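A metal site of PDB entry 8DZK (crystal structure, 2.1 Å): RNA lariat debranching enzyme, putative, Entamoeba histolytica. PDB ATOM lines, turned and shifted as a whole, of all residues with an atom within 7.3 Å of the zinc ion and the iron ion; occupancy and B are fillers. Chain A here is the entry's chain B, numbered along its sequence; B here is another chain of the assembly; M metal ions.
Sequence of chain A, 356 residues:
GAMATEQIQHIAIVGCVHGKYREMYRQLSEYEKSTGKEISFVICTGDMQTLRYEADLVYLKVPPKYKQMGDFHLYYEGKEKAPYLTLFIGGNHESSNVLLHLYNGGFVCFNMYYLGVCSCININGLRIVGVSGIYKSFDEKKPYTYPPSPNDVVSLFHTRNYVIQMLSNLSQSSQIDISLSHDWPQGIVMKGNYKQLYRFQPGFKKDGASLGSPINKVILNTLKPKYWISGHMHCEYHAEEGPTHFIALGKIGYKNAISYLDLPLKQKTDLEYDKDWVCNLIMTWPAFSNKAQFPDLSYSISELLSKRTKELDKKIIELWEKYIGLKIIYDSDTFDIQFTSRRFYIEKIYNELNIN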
ATOM      1  N   GLY A  15     -13.657  -6.468 -11.545  1.00  0.00           N
ATOM      2  CA  GLY A  15     -13.263  -5.981 -10.230  1.00  0.00           C
ATOM      3  C   GLY A  15     -12.909  -7.148  -9.322  1.00  0.00           C
ATOM      4  O   GLY A  15     -12.137  -8.028  -9.699  1.00  0.00           O
ATOM      5  N   CYS A  16     -13.458  -7.169  -8.125  1.00  0.00           N
ATOM      6  CA  CYS A  16     -13.108  -8.186  -7.146  1.00  0.00           C
ATOM      7  C   CYS A  16     -13.676  -9.551  -7.495  1.00  0.00           C
ATOM      8  O   CYS A  16     -14.883  -9.686  -7.719  1.00  0.00           O
ATOM      9  CB  CYS A  16     -13.624  -7.760  -5.779  1.00  0.00           C
ATOM     10  SG  CYS A  16     -12.975  -6.194  -5.232  1.00  0.00           S
ATOM     11  N   VAL A  17     -12.834 -10.573  -7.477  1.00  0.00           N
ATOM     12  CA  VAL A  17     -13.305 -11.936  -7.721  1.00  0.00           C
ATOM     13  C   VAL A  17     -13.684 -12.659  -6.431  1.00  0.00           C
ATOM     14  O   VAL A  17     -14.676 -13.390  -6.401  1.00  0.00           O
ATOM     15  CB  VAL A  17     -12.234 -12.711  -8.525  1.00  0.00           C
ATOM     16  CG1 VAL A  17     -12.628 -14.185  -8.661  1.00  0.00           C
ATOM     17  CG2 VAL A  17     -12.102 -12.085  -9.931  1.00  0.00           C
ATOM     18  N   HIS A  18     -12.898 -12.491  -5.351  1.00  0.00           N
ATOM     19  CA  HIS A  18     -13.160 -13.119  -4.046  1.00  0.00           C
ATOM     20  C   HIS A  18     -13.391 -14.615  -4.158  1.00  0.00           C
ATOM     21  O   HIS A  18     -14.310 -15.169  -3.557  1.00  0.00           O
ATOM     22  CB  HIS A  18     -14.343 -12.453  -3.339  1.00  0.00           C
ATOM     23  CG  HIS A  18     -14.047 -11.075  -2.871  1.00  0.00           C
ATOM     24  ND1 HIS A  18     -13.274 -10.825  -1.756  1.00  0.00           N
ATOM     25  CD2 HIS A  18     -14.383  -9.878  -3.383  1.00  0.00           C
ATOM     26  CE1 HIS A  18     -13.164  -9.514  -1.598  1.00  0.00           C
ATOM     27  NE2 HIS A  18     -13.834  -8.921  -2.565  1.00  0.00           N
ATOM     28  N   THR A  45      -8.826  -6.925 -11.196  1.00  0.00           N
ATOM     29  CA  THR A  45      -8.224  -5.927 -10.298  1.00  0.00           C
ATOM     30  C   THR A  45      -7.837  -6.397  -8.907  1.00  0.00           C
ATOM     31  O   THR A  45      -7.435  -5.584  -8.097  1.00  0.00           O
ATOM     32  CB  THR A  45      -9.154  -4.707 -10.190  1.00  0.00           C
ATOM     33  OG1 THR A  45     -10.482  -5.136  -9.913  1.00  0.00           O
ATOM     34  CG2 THR A  45      -9.136  -3.924 -11.474  1.00  0.00           C
ATOM     35  N   GLY A  46      -7.995  -7.668  -8.605  1.00  0.00           N
ATOM     36  CA  GLY A  46      -7.461  -8.174  -7.355  1.00  0.00           C
ATOM     37  C   GLY A  46      -8.504  -8.814  -6.460  1.00  0.00           C
ATOM     38  O   GLY A  46      -9.662  -9.022  -6.847  1.00  0.00           O
ATOM     39  N   ASP A  47      -8.077  -9.130  -5.236  1.00  0.00           N
ATOM     40  CA  ASP A  47      -8.825  -9.980  -4.309  1.00  0.00           C
ATOM     41  C   ASP A  47      -9.116 -11.353  -4.927  1.00  0.00           C
ATOM     42  O   ASP A  47     -10.243 -11.846  -4.891  1.00  0.00           O
ATOM     43  CB  ASP A  47     -10.115  -9.285  -3.827  1.00  0.00           C
ATOM     44  CG  ASP A  47      -9.832  -8.162  -2.859  1.00  0.00           C
ATOM     45  OD1 ASP A  47      -8.669  -8.072  -2.419  1.00  0.00           O
ATOM     46  OD2 ASP A  47     -10.741  -7.367  -2.526  1.00  0.00           O
ATOM     47  N   GLY A  91      -4.872  -7.909  -4.482  1.00  0.00           N
ATOM     48  CA  GLY A  91      -5.605  -6.938  -3.691  1.00  0.00           C
ATOM     49  C   GLY A  91      -5.274  -7.087  -2.227  1.00  0.00           C
ATOM     50  O   GLY A  91      -4.103  -7.288  -1.875  1.00  0.00           O
ATOM     51  N   ASN A  92      -6.276  -6.974  -1.350  1.00  0.00           N
ATOM     52  CA  ASN A  92      -6.085  -7.173   0.084  1.00  0.00           C
ATOM     53  C   ASN A  92      -6.635  -8.498   0.591  1.00  0.00           C
ATOM     54  O   ASN A  92      -6.477  -8.788   1.779  1.00  0.00           O
ATOM     55  CB  ASN A  92      -6.722  -6.019   0.863  1.00  0.00           C
ATOM     56  CG  ASN A  92      -8.184  -5.845   0.528  1.00  0.00           C
ATOM     57  OD1 ASN A  92      -8.533  -5.533  -0.604  1.00  0.00           O
ATOM     58  ND2 ASN A  92      -9.042  -6.071   1.494  1.00  0.00           N
ATOM     59  N   HIS A  93      -7.277  -9.294  -0.250  1.00  0.00           N
ATOM     60  CA  HIS A  93      -7.721 -10.641   0.146  1.00  0.00           C
ATOM     61  C   HIS A  93      -7.015 -11.620  -0.791  1.00  0.00           C
ATOM     62  O   HIS A  93      -7.542 -11.961  -1.852  1.00  0.00           O
ATOM     63  CB  HIS A  93      -9.228 -10.800   0.066  1.00  0.00           C
ATOM     64  CG  HIS A  93      -9.975  -9.944   1.044  1.00  0.00           C
ATOM     65  ND1 HIS A  93      -9.501  -9.662   2.309  1.00  0.00           N
ATOM     66  CD2 HIS A  93     -11.149  -9.265   0.918  1.00  0.00           C
ATOM     67  CE1 HIS A  93     -10.360  -8.871   2.926  1.00  0.00           C
ATOM     68  NE2 HIS A  93     -11.365  -8.614   2.112  1.00  0.00           N
ATOM     69  N   GLU A  94      -5.811 -12.039  -0.399  1.00  0.00           N
ATOM     70  CA  GLU A  94      -4.929 -12.818  -1.247  1.00  0.00           C
ATOM     71  C   GLU A  94      -4.274 -13.924  -0.427  1.00  0.00           C
ATOM     72  O   GLU A  94      -4.096 -13.805   0.790  1.00  0.00           O
ATOM     73  CB  GLU A  94      -3.836 -11.914  -1.845  1.00  0.00           C
ATOM     74  CG  GLU A  94      -4.350 -10.792  -2.743  1.00  0.00           C
ATOM     75  CD  GLU A  94      -5.123 -11.238  -3.990  1.00  0.00           C
ATOM     76  OE1 GLU A  94      -5.142 -12.456  -4.348  1.00  0.00           O
ATOM     77  OE2 GLU A  94      -5.762 -10.349  -4.601  1.00  0.00           O
ATOM     78  N   ILE A 134      -3.029  -2.689  -1.421  1.00  0.00           N
ATOM     79  CA  ILE A 134      -3.713  -1.467  -1.008  1.00  0.00           C
ATOM     80  C   ILE A 134      -2.757  -0.664  -0.116  1.00  0.00           C
ATOM     81  O   ILE A 134      -1.871  -1.208   0.533  1.00  0.00           O
ATOM     82  CB  ILE A 134      -5.052  -1.714  -0.281  1.00  0.00           C
ATOM     83  CG1 ILE A 134      -4.818  -2.349   1.093  1.00  0.00           C
ATOM     84  CG2 ILE A 134      -6.001  -2.521  -1.127  1.00  0.00           C
ATOM     85  CD1 ILE A 134      -6.058  -2.405   1.953  1.00  0.00           C
ATOM     86  N   HIS A 182      -5.533  -2.061  -7.311  1.00  0.00           N
ATOM     87  CA  HIS A 182      -6.668  -2.572  -6.564  1.00  0.00           C
ATOM     88  C   HIS A 182      -7.464  -1.436  -5.928  1.00  0.00           C
ATOM     89  O   HIS A 182      -8.625  -1.221  -6.284  1.00  0.00           O
ATOM     90  CB  HIS A 182      -6.222  -3.584  -5.513  1.00  0.00           C
ATOM     91  CG  HIS A 182      -7.385  -4.241  -4.866  1.00  0.00           C
ATOM     92  ND1 HIS A 182      -8.312  -4.967  -5.588  1.00  0.00           N
ATOM     93  CD2 HIS A 182      -7.828  -4.244  -3.586  1.00  0.00           C
ATOM     94  CE1 HIS A 182      -9.261  -5.397  -4.780  1.00  0.00           C
ATOM     95  NE2 HIS A 182      -8.983  -4.983  -3.565  1.00  0.00           N
ATOM     96  N   ASP A 183      -6.840  -0.687  -5.028  1.00  0.00           N
ATOM     97  CA  ASP A 183      -7.548   0.476  -4.510  1.00  0.00           C
ATOM     98  C   ASP A 183      -7.423   1.641  -5.482  1.00  0.00           C
ATOM     99  O   ASP A 183      -6.567   1.642  -6.392  1.00  0.00           O
ATOM    100  CB  ASP A 183      -7.101   0.853  -3.088  1.00  0.00           C
ATOM    101  CG  ASP A 183      -5.585   1.049  -2.941  1.00  0.00           C
ATOM    102  OD1 ASP A 183      -4.802   0.719  -3.862  1.00  0.00           O
ATOM    103  OD2 ASP A 183      -5.168   1.561  -1.855  1.00  0.00           O
ATOM    104  N   GLY A 231     -10.573  -1.671  -8.550  1.00  0.00           N
ATOM    105  CA  GLY A 231     -11.680  -2.370  -7.928  1.00  0.00           C
ATOM    106  C   GLY A 231     -11.843  -1.890  -6.505  1.00  0.00           C
ATOM    107  O   GLY A 231     -11.881  -0.692  -6.213  1.00  0.00           O
ATOM    108  N   HIS A 232     -12.018  -2.861  -5.616  1.00  0.00           N
ATOM    109  CA  HIS A 232     -11.896  -2.768  -4.164  1.00  0.00           C
ATOM    110  C   HIS A 232     -13.014  -1.996  -3.482  1.00  0.00           C
ATOM    111  O   HIS A 232     -13.308  -2.264  -2.314  1.00  0.00           O
ATOM    112  CB  HIS A 232     -10.555  -2.105  -3.777  1.00  0.00           C
ATOM    113  CG  HIS A 232     -10.329  -1.953  -2.295  1.00  0.00           C
ATOM    114  ND1 HIS A 232     -10.295  -3.030  -1.424  1.00  0.00           N
ATOM    115  CD2 HIS A 232     -10.048  -0.862  -1.544  1.00  0.00           C
ATOM    116  CE1 HIS A 232     -10.036  -2.595  -0.201  1.00  0.00           C
ATOM    117  NE2 HIS A 232      -9.883  -1.282  -0.245  1.00  0.00           N
ATOM    118  N   MET A 233     -13.718  -1.139  -4.207  1.00  0.00           N
ATOM    119  CA  MET A 233     -14.738  -0.284  -3.609  1.00  0.00           C
ATOM    120  C   MET A 233     -16.139  -0.841  -3.814  1.00  0.00           C
ATOM    121  O   MET A 233     -17.099  -0.290  -3.264  1.00  0.00           O
ATOM    122  CB  MET A 233     -14.650   1.132  -4.184  1.00  0.00           C
ATOM    123  CG  MET A 233     -13.608   2.106  -3.583  1.00  0.00           C
ATOM    124  SD  MET A 233     -12.939   1.846  -1.933  1.00  0.00           S
ATOM    125  CE  MET A 233     -14.309   2.490  -0.987  1.00  0.00           C
ATOM    126  N   HIS A 234     -16.279  -1.905  -4.606  1.00  0.00           N
ATOM    127  CA  HIS A 234     -17.534  -2.632  -4.783  1.00  0.00           C
ATOM    128  C   HIS A 234     -18.618  -1.750  -5.406  1.00  0.00           C
ATOM    129  O   HIS A 234     -19.798  -1.875  -5.096  1.00  0.00           O
ATOM    130  CB  HIS A 234     -18.001  -3.243  -3.438  1.00  0.00           C
ATOM    131  CG  HIS A 234     -17.068  -4.297  -2.901  1.00  0.00           C
ATOM    132  ND1 HIS A 234     -17.172  -4.814  -1.625  1.00  0.00           N
ATOM    133  CD2 HIS A 234     -16.017  -4.941  -3.480  1.00  0.00           C
ATOM    134  CE1 HIS A 234     -16.218  -5.719  -1.439  1.00  0.00           C
ATOM    135  NE2 HIS A 234     -15.503  -5.825  -2.540  1.00  0.00           N
ATOM    136  N   GLY A 250     -17.083  -3.286  -9.711  1.00  0.00           N
ATOM    137  CA  GLY A 250     -17.599  -3.966  -8.530  1.00  0.00           C
ATOM    138  C   GLY A 250     -17.074  -5.388  -8.370  1.00  0.00           C
ATOM    139  O   GLY A 250     -16.080  -5.785  -8.988  1.00  0.00           O
ATOM    140  N   LYS A 251     -17.754  -6.176  -7.536  1.00  0.00           N
ATOM    141  CA  LYS A 251     -17.310  -7.535  -7.245  1.00  0.00           C
ATOM    142  C   LYS A 251     -18.194  -8.571  -7.935  1.00  0.00           C
ATOM    143  O   LYS A 251     -19.381  -8.335  -8.186  1.00  0.00           O
ATOM    144  CB  LYS A 251     -17.258  -7.842  -5.735  1.00  0.00           C
ATOM    145  CG  LYS A 251     -18.511  -7.535  -4.966  1.00  0.00           C
ATOM    146  CD  LYS A 251     -18.407  -8.050  -3.531  1.00  0.00           C
ATOM    147  CE  LYS A 251     -18.583  -9.562  -3.476  1.00  0.00           C
ATOM    148  NZ  LYS A 251     -18.649 -10.131  -2.093  1.00  0.00           N
ATOM    149  P   G46 B   1     -12.426  -5.583   0.001  1.00  0.00           P
ATOM    150  O1P G46 B   1     -11.140  -6.067   0.545  1.00  0.00           O
ATOM    151  S2P G46 B   1     -13.840  -7.060   0.182  1.00  0.00           S
ATOM    152  O3P G46 B   1     -12.224  -5.132  -1.540  1.00  0.00           O
ATOM    153  O5' G46 B   1     -12.845  -4.251   0.769  1.00  0.00           O
ATOM    154  C5' G46 B   1     -14.050  -3.607   0.402  1.00  0.00           C
ATOM    155  C4' G46 B   1     -14.552  -2.842   1.607  1.00  0.00           C
ATOM    156  O4' G46 B   1     -13.579  -1.902   2.053  1.00  0.00           O
ATOM    157  C3' G46 B   1     -15.794  -2.093   1.190  1.00  0.00           C
ATOM    158  O3' G46 B   1     -16.850  -2.497   2.075  1.00  0.00           O
ATOM    159  C2' G46 B   1     -15.422  -0.625   1.331  1.00  0.00           C
ATOM    160  C1' G46 B   1     -14.206  -0.628   2.251  1.00  0.00           C
ATOM    161  O2' G46 B   1     -16.494   0.149   1.886  1.00  0.00           O
ATOM    162  N9  G46 B   1     -13.233   0.467   1.962  1.00  0.00           N
ATOM    163  C8  G46 B   1     -11.976   0.279   1.540  1.00  0.00           C
ATOM    164  N7  G46 B   1     -11.316   1.450   1.381  1.00  0.00           N
ATOM    165  C5  G46 B   1     -12.166   2.435   1.719  1.00  0.00           C
ATOM    166  C6  G46 B   1     -12.099   3.912   1.769  1.00  0.00           C
ATOM    167  O6  G46 B   1     -11.047   4.517   1.452  1.00  0.00           O
ATOM    168  N1  G46 B   1     -13.197   4.573   2.176  1.00  0.00           N
ATOM    169  C2  G46 B   1     -14.336   3.932   2.524  1.00  0.00           C
ATOM    170  N2  G46 B   1     -15.407   4.678   2.920  1.00  0.00           N
ATOM    171  N3  G46 B   1     -14.461   2.575   2.500  1.00  0.00           N
ATOM    172  C4  G46 B   1     -13.429   1.780   2.117  1.00  0.00           C
ATOM    173  P     U B   2     -17.481  -3.912   2.585  1.00  0.00           P
ATOM    174  OP1   U B   2     -18.019  -4.838   1.555  1.00  0.00           O
ATOM    175  OP2   U B   2     -18.415  -3.306   3.562  1.00  0.00           O
ATOM    176  O5'   U B   2     -16.350  -4.692   3.403  1.00  0.00           O
ATOM    177  C5'   U B   2     -16.501  -4.995   4.778  1.00  0.00           C
ATOM    178  C4'   U B   2     -15.396  -5.890   5.290  1.00  0.00           C
ATOM    179  O4'   U B   2     -15.635  -7.258   4.853  1.00  0.00           O
ATOM    180  C3'   U B   2     -13.990  -5.537   4.806  1.00  0.00           C
ATOM    181  O3'   U B   2     -13.035  -5.846   5.829  1.00  0.00           O
ATOM    182  C2'   U B   2     -13.788  -6.481   3.633  1.00  0.00           C
ATOM    183  O2'   U B   2     -12.429  -6.752   3.321  1.00  0.00           O
ATOM    184  C1'   U B   2     -14.511  -7.735   4.121  1.00  0.00           C
ATOM    185  N1    U B   2     -14.978  -8.622   3.037  1.00  0.00           N
ATOM    186  C2    U B   2     -16.137  -8.326   2.317  1.00  0.00           C
ATOM    187  O2    U B   2     -16.847  -7.348   2.506  1.00  0.00           O
ATOM    188  N3    U B   2     -16.454  -9.233   1.326  1.00  0.00           N
ATOM    189  C4    U B   2     -15.768 -10.376   0.989  1.00  0.00           C
ATOM    190  O4    U B   2     -16.194 -11.088   0.078  1.00  0.00           O
ATOM    191  C5    U B   2     -14.592 -10.622   1.772  1.00  0.00           C
ATOM    192  C6    U B   2     -14.251  -9.756   2.742  1.00  0.00           C
ATOM    193  P     G B   3     -11.971  -4.734   6.308  1.00  0.00           P
ATOM    194  OP1   G B   3     -10.782  -5.455   6.842  1.00  0.00           O
ATOM    195  OP2   G B   3     -12.688  -3.770   7.174  1.00  0.00           O
ATOM    196  O5'   G B   3     -11.544  -3.987   4.963  1.00  0.00           O
ATOM    197  C5'   G B   3     -10.440  -4.452   4.185  1.00  0.00           C
ATOM    198  C4'   G B   3      -9.301  -3.457   4.168  1.00  0.00           C
ATOM    199  O4'   G B   3      -9.807  -2.152   3.785  1.00  0.00           O
ATOM    200  C3'   G B   3      -8.598  -3.267   5.515  1.00  0.00           C
ATOM    201  O3'   G B   3      -7.200  -3.024   5.316  1.00  0.00           O
ATOM    202  C2'   G B   3      -9.237  -1.994   6.066  1.00  0.00           C
ATOM    203  O2'   G B   3      -8.427  -1.280   6.971  1.00  0.00           O
ATOM    204  C1'   G B   3      -9.476  -1.196   4.780  1.00  0.00           C
ATOM    205  N9    G B   3     -10.566  -0.236   4.910  1.00  0.00           N
ATOM    206  C8    G B   3     -11.915  -0.490   5.056  1.00  0.00           C
ATOM    207  N7    G B   3     -12.628   0.610   5.157  1.00  0.00           N
ATOM    208  C5    G B   3     -11.692   1.631   5.076  1.00  0.00           C
ATOM    209  C6    G B   3     -11.856   3.031   5.123  1.00  0.00           C
ATOM    210  O6    G B   3     -12.903   3.671   5.250  1.00  0.00           O
ATOM    211  N1    G B   3     -10.641   3.698   5.010  1.00  0.00           N
ATOM    212  C2    G B   3      -9.404   3.098   4.859  1.00  0.00           C
ATOM    213  N2    G B   3      -8.340   3.896   4.761  1.00  0.00           N
ATOM    214  N3    G B   3      -9.246   1.783   4.809  1.00  0.00           N
ATOM    215  C4    G B   3     -10.420   1.128   4.929  1.00  0.00           C
HETATM  216 ZN    ZN M   1     -13.383  -6.713  -2.987  1.00  0.00          ZN
HETATM  217 FE    FE M   2     -10.159  -5.286  -1.827  1.00  0.00          FE
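NE2 of His 93 sits at hydrogen-bond distance from O1P of G46 1 of chain B.
The backbone carbonyl oxygen of His 182 is in hydrogen-bond range of the backbone NH of Gly 231, at 3.0 Å.
The backbone carbonyl oxygen of Thr 45 lies within hydrogen-bond range of a ring nitrogen (ND1) of His 182, 2.7 Å away.
O of Asp 47 sits at hydrogen-bond distance from N of His 18.
The backbone NH (N) of Asp 47 is in hydrogen-bond range of the side-chain carboxylate (OE2) of Glu 94.
N of His 232 lies close to SG of Cys 16, 3.5 Å away.
O of Gly 250 is in hydrogen-bond range of N of Cys 16 (3.1 Å).
OP1 of U 2 of chain B lies within hydrogen-bond range of a ring nitrogen (ND1) of His 234, at 3.3 Å.
Of the 23 residues printed, 5 come within 4 Å of the zinc ion.
Along chain A the residues within 4 Å of the zinc ion span positions 16 to 234.
Within 4 Å of the iron ion: Asp 47, Asn 92, His 182, His 232 and G46 1 of chain B.
The zinc ion is bound by NE2 of His 18 (2.3 Å), SG of Cys 16 (2.3 Å), NE2 of His 234 (2.3 Å) and O3P of G46 1 of chain B (2.4 Å).
The zinc ion has four donor atoms within binding distance.
Slightly farther from the zinc ion lies OD2 of Asp 47 (2.8 Å).
The iron ion is bound by OD1 of Asn 92, O3P of G46 1 of chain B, NE2 of His 182, OD2 of Asp 47 and ND1 of His 232.
Slightly farther from the iron ion lies O1P of G46 1 of chain B (2.7 Å).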
